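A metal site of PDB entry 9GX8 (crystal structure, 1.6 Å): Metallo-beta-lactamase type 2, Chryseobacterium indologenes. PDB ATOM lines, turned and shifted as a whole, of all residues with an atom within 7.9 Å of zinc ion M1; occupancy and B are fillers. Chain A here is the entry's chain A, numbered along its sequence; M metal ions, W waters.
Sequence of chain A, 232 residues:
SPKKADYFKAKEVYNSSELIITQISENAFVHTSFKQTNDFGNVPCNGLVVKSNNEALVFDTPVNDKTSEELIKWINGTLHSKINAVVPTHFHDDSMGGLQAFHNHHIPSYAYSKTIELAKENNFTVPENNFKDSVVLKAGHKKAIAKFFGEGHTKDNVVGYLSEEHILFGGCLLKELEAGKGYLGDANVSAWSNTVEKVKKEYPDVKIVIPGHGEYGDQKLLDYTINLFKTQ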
ATOM      1  N   LYS A  35      19.571 -16.165  16.189  1.00  0.00           N
ATOM      2  CA  LYS A  35      20.211 -15.119  15.414  1.00  0.00           C
ATOM      3  C   LYS A  35      20.036 -13.803  16.147  1.00  0.00           C
ATOM      4  O   LYS A  35      18.908 -13.396  16.441  1.00  0.00           O
ATOM      5  CB  LYS A  35      19.605 -15.057  14.014  1.00  0.00           C
ATOM      6  CG  LYS A  35      20.048 -13.888  13.167  1.00  0.00           C
ATOM      7  CD  LYS A  35      19.350 -13.931  11.816  1.00  0.00           C
ATOM      8  CE  LYS A  35      19.653 -12.684  10.998  1.00  0.00           C
ATOM      9  NZ  LYS A  35      21.108 -12.399  10.849  1.00  0.00           N
ATOM     10  N   HIS A  90      15.422 -21.201   2.153  1.00  0.00           N
ATOM     11  CA  HIS A  90      15.623 -19.964   1.389  1.00  0.00           C
ATOM     12  C   HIS A  90      17.023 -19.447   1.700  1.00  0.00           C
ATOM     13  O   HIS A  90      17.761 -20.051   2.475  1.00  0.00           O
ATOM     14  CB  HIS A  90      14.534 -18.934   1.669  1.00  0.00           C
ATOM     15  CG  HIS A  90      14.610 -18.291   3.012  1.00  0.00           C
ATOM     16  ND1 HIS A  90      14.632 -18.997   4.202  1.00  0.00           N
ATOM     17  CD2 HIS A  90      14.607 -16.979   3.363  1.00  0.00           C
ATOM     18  CE1 HIS A  90      14.664 -18.155   5.217  1.00  0.00           C
ATOM     19  NE2 HIS A  90      14.646 -16.923   4.731  1.00  0.00           N
ATOM     20  N   PHE A  91      17.400 -18.339   1.050  1.00  0.00           N
ATOM     21  CA  PHE A  91      18.817 -17.982   1.041  1.00  0.00           C
ATOM     22  C   PHE A  91      19.277 -17.211   2.283  1.00  0.00           C
ATOM     23  O   PHE A  91      20.486 -17.049   2.455  1.00  0.00           O
ATOM     24  CB  PHE A  91      19.139 -17.161  -0.231  1.00  0.00           C
ATOM     25  CG  PHE A  91      18.672 -15.727  -0.188  1.00  0.00           C
ATOM     26  CD1 PHE A  91      17.350 -15.398  -0.449  1.00  0.00           C
ATOM     27  CD2 PHE A  91      19.566 -14.707   0.107  1.00  0.00           C
ATOM     28  CE1 PHE A  91      16.917 -14.079  -0.420  1.00  0.00           C
ATOM     29  CE2 PHE A  91      19.158 -13.373   0.137  1.00  0.00           C
ATOM     30  CZ  PHE A  91      17.824 -13.061  -0.131  1.00  0.00           C
ATOM     31  N   HIS A  92      18.370 -16.713   3.119  1.00  0.00           N
ATOM     32  CA  HIS A  92      18.786 -15.983   4.311  1.00  0.00           C
ATOM     33  C   HIS A  92      19.566 -16.891   5.266  1.00  0.00           C
ATOM     34  O   HIS A  92      19.453 -18.110   5.224  1.00  0.00           O
ATOM     35  CB  HIS A  92      17.575 -15.413   5.039  1.00  0.00           C
ATOM     36  CG  HIS A  92      16.894 -14.300   4.304  1.00  0.00           C
ATOM     37  ND1 HIS A  92      15.627 -13.874   4.611  1.00  0.00           N
ATOM     38  CD2 HIS A  92      17.329 -13.497   3.309  1.00  0.00           C
ATOM     39  CE1 HIS A  92      15.281 -12.870   3.819  1.00  0.00           C
ATOM     40  NE2 HIS A  92      16.313 -12.621   3.024  1.00  0.00           N
ATOM     41  N   ASP A  93      20.339 -16.267   6.168  1.00  0.00           N
ATOM     42  CA  ASP A  93      21.224 -17.066   6.996  1.00  0.00           C
ATOM     43  C   ASP A  93      20.449 -17.941   7.963  1.00  0.00           C
ATOM     44  O   ASP A  93      20.977 -18.966   8.383  1.00  0.00           O
ATOM     45  CB  ASP A  93      22.235 -16.206   7.773  1.00  0.00           C
ATOM     46  CG  ASP A  93      21.591 -15.130   8.621  1.00  0.00           C
ATOM     47  OD1 ASP A  93      20.391 -14.857   8.456  1.00  0.00           O
ATOM     48  OD2 ASP A  93      22.312 -14.553   9.471  1.00  0.00           O
ATOM     49  N   ASP A  94      19.204 -17.595   8.308  1.00  0.00           N
ATOM     50  CA  ASP A  94      18.518 -18.479   9.249  1.00  0.00           C
ATOM     51  C   ASP A  94      17.945 -19.736   8.586  1.00  0.00           C
ATOM     52  O   ASP A  94      17.352 -20.560   9.282  1.00  0.00           O
ATOM     53  CB  ASP A  94      17.406 -17.747  10.016  1.00  0.00           C
ATOM     54  CG  ASP A  94      16.405 -17.060   9.114  1.00  0.00           C
ATOM     55  OD1 ASP A  94      16.825 -16.263   8.246  1.00  0.00           O
ATOM     56  OD2 ASP A  94      15.201 -17.319   9.279  1.00  0.00           O
ATOM     57  N   SER A  95      18.130 -19.899   7.278  1.00  0.00           N
ATOM     58  CA  SER A  95      17.949 -21.189   6.629  1.00  0.00           C
ATOM     59  C   SER A  95      19.199 -21.733   5.981  1.00  0.00           C
ATOM     60  O   SER A  95      19.265 -22.944   5.728  1.00  0.00           O
ATOM     61  CB  SER A  95      16.845 -21.140   5.550  1.00  0.00           C
ATOM     62  OG  SER A  95      15.578 -20.794   6.106  1.00  0.00           O
ATOM     63  N   HIS A 153       7.680 -14.740   1.646  1.00  0.00           N
ATOM     64  CA  HIS A 153       8.736 -14.199   2.490  1.00  0.00           C
ATOM     65  C   HIS A 153       9.952 -13.805   1.666  1.00  0.00           C
ATOM     66  O   HIS A 153      10.573 -12.754   1.916  1.00  0.00           O
ATOM     67  CB  HIS A 153       9.116 -15.225   3.558  1.00  0.00           C
ATOM     68  CG  HIS A 153      10.299 -14.814   4.355  1.00  0.00           C
ATOM     69  ND1 HIS A 153      10.248 -13.803   5.276  1.00  0.00           N
ATOM     70  CD2 HIS A 153      11.571 -15.253   4.343  1.00  0.00           C
ATOM     71  CE1 HIS A 153      11.429 -13.644   5.824  1.00  0.00           C
ATOM     72  NE2 HIS A 153      12.257 -14.504   5.260  1.00  0.00           N
ATOM     73  N   THR A 154      10.334 -14.645   0.707  1.00  0.00           N
ATOM     74  CA  THR A 154      11.335 -14.287  -0.293  1.00  0.00           C
ATOM     75  C   THR A 154      10.845 -14.801  -1.639  1.00  0.00           C
ATOM     76  O   THR A 154       9.806 -15.455  -1.730  1.00  0.00           O
ATOM     77  CB  THR A 154      12.715 -14.878   0.032  1.00  0.00           C
ATOM     78  OG1 THR A 154      12.568 -16.281   0.280  1.00  0.00           O
ATOM     79  CG2 THR A 154      13.358 -14.179   1.235  1.00  0.00           C
ATOM     80  N   ASP A 156      12.384 -17.028  -3.276  1.00  0.00           N
ATOM     81  CA  ASP A 156      12.906 -18.366  -3.451  1.00  0.00           C
ATOM     82  C   ASP A 156      12.383 -19.357  -2.427  1.00  0.00           C
ATOM     83  O   ASP A 156      12.773 -20.523  -2.473  1.00  0.00           O
ATOM     84  CB  ASP A 156      14.439 -18.349  -3.369  1.00  0.00           C
ATOM     85  CG  ASP A 156      14.951 -17.934  -1.998  1.00  0.00           C
ATOM     86  OD1 ASP A 156      14.450 -16.940  -1.435  1.00  0.00           O
ATOM     87  OD2 ASP A 156      15.856 -18.624  -1.470  1.00  0.00           O
ATOM     88  N   ASN A 157      11.516 -18.932  -1.516  1.00  0.00           N
ATOM     89  CA  ASN A 157      11.238 -19.778  -0.366  1.00  0.00           C
ATOM     90  C   ASN A 157      10.495 -21.040  -0.782  1.00  0.00           C
ATOM     91  O   ASN A 157       9.583 -21.001  -1.619  1.00  0.00           O
ATOM     92  CB  ASN A 157      10.479 -18.999   0.725  1.00  0.00           C
ATOM     93  CG  ASN A 157       9.254 -18.225   0.242  1.00  0.00           C
ATOM     94  OD1 ASN A 157       8.819 -17.313   0.941  1.00  0.00           O
ATOM     95  ND2 ASN A 157       8.685 -18.583  -0.904  1.00  0.00           N
ATOM     96  N   GLY A 171       8.986 -23.269   6.740  1.00  0.00           N
ATOM     97  CA  GLY A 171      10.056 -22.300   6.658  1.00  0.00           C
ATOM     98  C   GLY A 171       9.526 -20.899   6.955  1.00  0.00           C
ATOM     99  O   GLY A 171       8.475 -20.707   7.567  1.00  0.00           O
ATOM    100  N   CYS A 172      10.264 -19.903   6.465  1.00  0.00           N
ATOM    101  CA  CYS A 172       9.892 -18.540   6.832  1.00  0.00           C
ATOM    102  C   CYS A 172       8.701 -18.014   6.039  1.00  0.00           C
ATOM    103  O   CYS A 172       8.208 -16.931   6.331  1.00  0.00           O
ATOM    104  CB  CYS A 172      11.098 -17.639   6.704  1.00  0.00           C
ATOM    105  SG  CYS A 172      12.357 -18.117   7.899  1.00  0.00           S
ATOM    106  N   LEU A 173       8.227 -18.780   5.058  1.00  0.00           N
ATOM    107  CA  LEU A 173       6.949 -18.514   4.422  1.00  0.00           C
ATOM    108  C   LEU A 173       5.792 -18.645   5.394  1.00  0.00           C
ATOM    109  O   LEU A 173       4.731 -18.033   5.185  1.00  0.00           O
ATOM    110  CB  LEU A 173       6.767 -19.484   3.246  1.00  0.00           C
ATOM    111  CG  LEU A 173       5.459 -19.370   2.477  1.00  0.00           C
ATOM    112  CD1 LEU A 173       5.540 -18.152   1.553  1.00  0.00           C
ATOM    113  CD2 LEU A 173       5.214 -20.637   1.662  1.00  0.00           C
ATOM    114  N   LYS A 175       4.199 -18.221   9.227  1.00  0.00           N
ATOM    115  CA  LYS A 175       4.283 -17.508  10.501  1.00  0.00           C
ATOM    116  C   LYS A 175       3.696 -18.340  11.633  1.00  0.00           C
ATOM    117  O   LYS A 175       2.743 -19.091  11.431  1.00  0.00           O
ATOM    118  CB  LYS A 175       3.536 -16.180  10.433  1.00  0.00           C
ATOM    119  CG  LYS A 175       4.123 -15.182   9.429  1.00  0.00           C
ATOM    120  CD  LYS A 175       5.553 -14.820   9.799  1.00  0.00           C
ATOM    121  CE  LYS A 175       6.082 -13.729   8.867  1.00  0.00           C
ATOM    122  NZ  LYS A 175       7.507 -13.375   9.208  1.00  0.00           N
ATOM    123  N   TYR A 183      10.424  -9.420   8.726  1.00  0.00           N
ATOM    124  CA  TYR A 183      11.282  -8.708   7.781  1.00  0.00           C
ATOM    125  C   TYR A 183      10.743  -8.857   6.363  1.00  0.00           C
ATOM    126  O   TYR A 183      10.609  -9.982   5.861  1.00  0.00           O
ATOM    127  CB  TYR A 183      12.719  -9.235   7.864  1.00  0.00           C
ATOM    128  CG  TYR A 183      13.632  -8.628   6.827  1.00  0.00           C
ATOM    129  CD1 TYR A 183      14.154  -9.404   5.798  1.00  0.00           C
ATOM    130  CD2 TYR A 183      13.962  -7.282   6.865  1.00  0.00           C
ATOM    131  CE1 TYR A 183      14.986  -8.842   4.834  1.00  0.00           C
ATOM    132  CE2 TYR A 183      14.788  -6.712   5.922  1.00  0.00           C
ATOM    133  CZ  TYR A 183      15.300  -7.492   4.907  1.00  0.00           C
ATOM    134  OH  TYR A 183      16.131  -6.893   3.983  1.00  0.00           O
ATOM    135  N   ASP A 186      12.919  -8.580   1.423  1.00  0.00           N
ATOM    136  CA  ASP A 186      13.044  -9.481   0.286  1.00  0.00           C
ATOM    137  C   ASP A 186      11.724 -10.128  -0.105  1.00  0.00           C
ATOM    138  O   ASP A 186      11.718 -11.007  -0.965  1.00  0.00           O
ATOM    139  CB  ASP A 186      14.103 -10.547   0.562  1.00  0.00           C
ATOM    140  CG  ASP A 186      15.489  -9.954   0.715  1.00  0.00           C
ATOM    141  OD1 ASP A 186      15.855  -9.053  -0.074  1.00  0.00           O
ATOM    142  OD2 ASP A 186      16.217 -10.377   1.631  1.00  0.00           O
ATOM    143  N   HIS A 213      10.086 -19.300  12.437  1.00  0.00           N
ATOM    144  CA  HIS A 213      10.379 -18.725  13.744  1.00  0.00           C
ATOM    145  C   HIS A 213       9.203 -18.957  14.665  1.00  0.00           C
ATOM    146  O   HIS A 213       8.064 -18.653  14.296  1.00  0.00           O
ATOM    147  CB  HIS A 213      10.641 -17.214  13.655  1.00  0.00           C
ATOM    148  CG  HIS A 213      11.712 -16.860  12.690  1.00  0.00           C
ATOM    149  ND1 HIS A 213      13.051 -17.025  12.982  1.00  0.00           N
ATOM    150  CD2 HIS A 213      11.663 -16.377  11.431  1.00  0.00           C
ATOM    151  CE1 HIS A 213      13.778 -16.633  11.952  1.00  0.00           C
ATOM    152  NE2 HIS A 213      12.960 -16.234  11.000  1.00  0.00           N
HETATM  153 ZN    ZN M   1      14.266 -15.093   5.791  1.00  0.00          ZN
HETATM  154 ZN    ZN M   2      13.281 -16.235   8.779  1.00  0.00          ZN
HETATM  155  O   HOH W   1      14.383 -14.838   7.650  1.00  0.00           O
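Zinc ion M1 is bound by water W1 (1.9 Å), a ring nitrogen (NE2) of His 90 (2.1 Å), a ring nitrogen (NE2) of His 153 (2.2 Å) and a ring nitrogen (ND1) of His 92 (2.2 Å).
Zinc ion M1 has four donor atoms within binding distance.
The side-chain hydroxyl (OG) of Ser 95 sits at hydrogen-bond distance from a ring nitrogen (ND1) of His 90 (2.8 Å).
The side-chain amide oxygen (OD1) of Asn 157 sits at hydrogen-bond distance from the backbone NH (N) of His 153 (2.9 Å).
The side-chain carboxylate (OD2) of Asp 186 is in hydrogen-bond range of a ring nitrogen (NE2) of His 92 (2.6 Å).
Asp 94 touches zinc ion M1 (OD1 to ZN, 3.7 Å).
Of the 18 residues printed, 4 come within 4 Å of zinc ion M1.
The nearest printed residue that does not touch zinc ion M1 is Cys 172 (4.2 Å).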
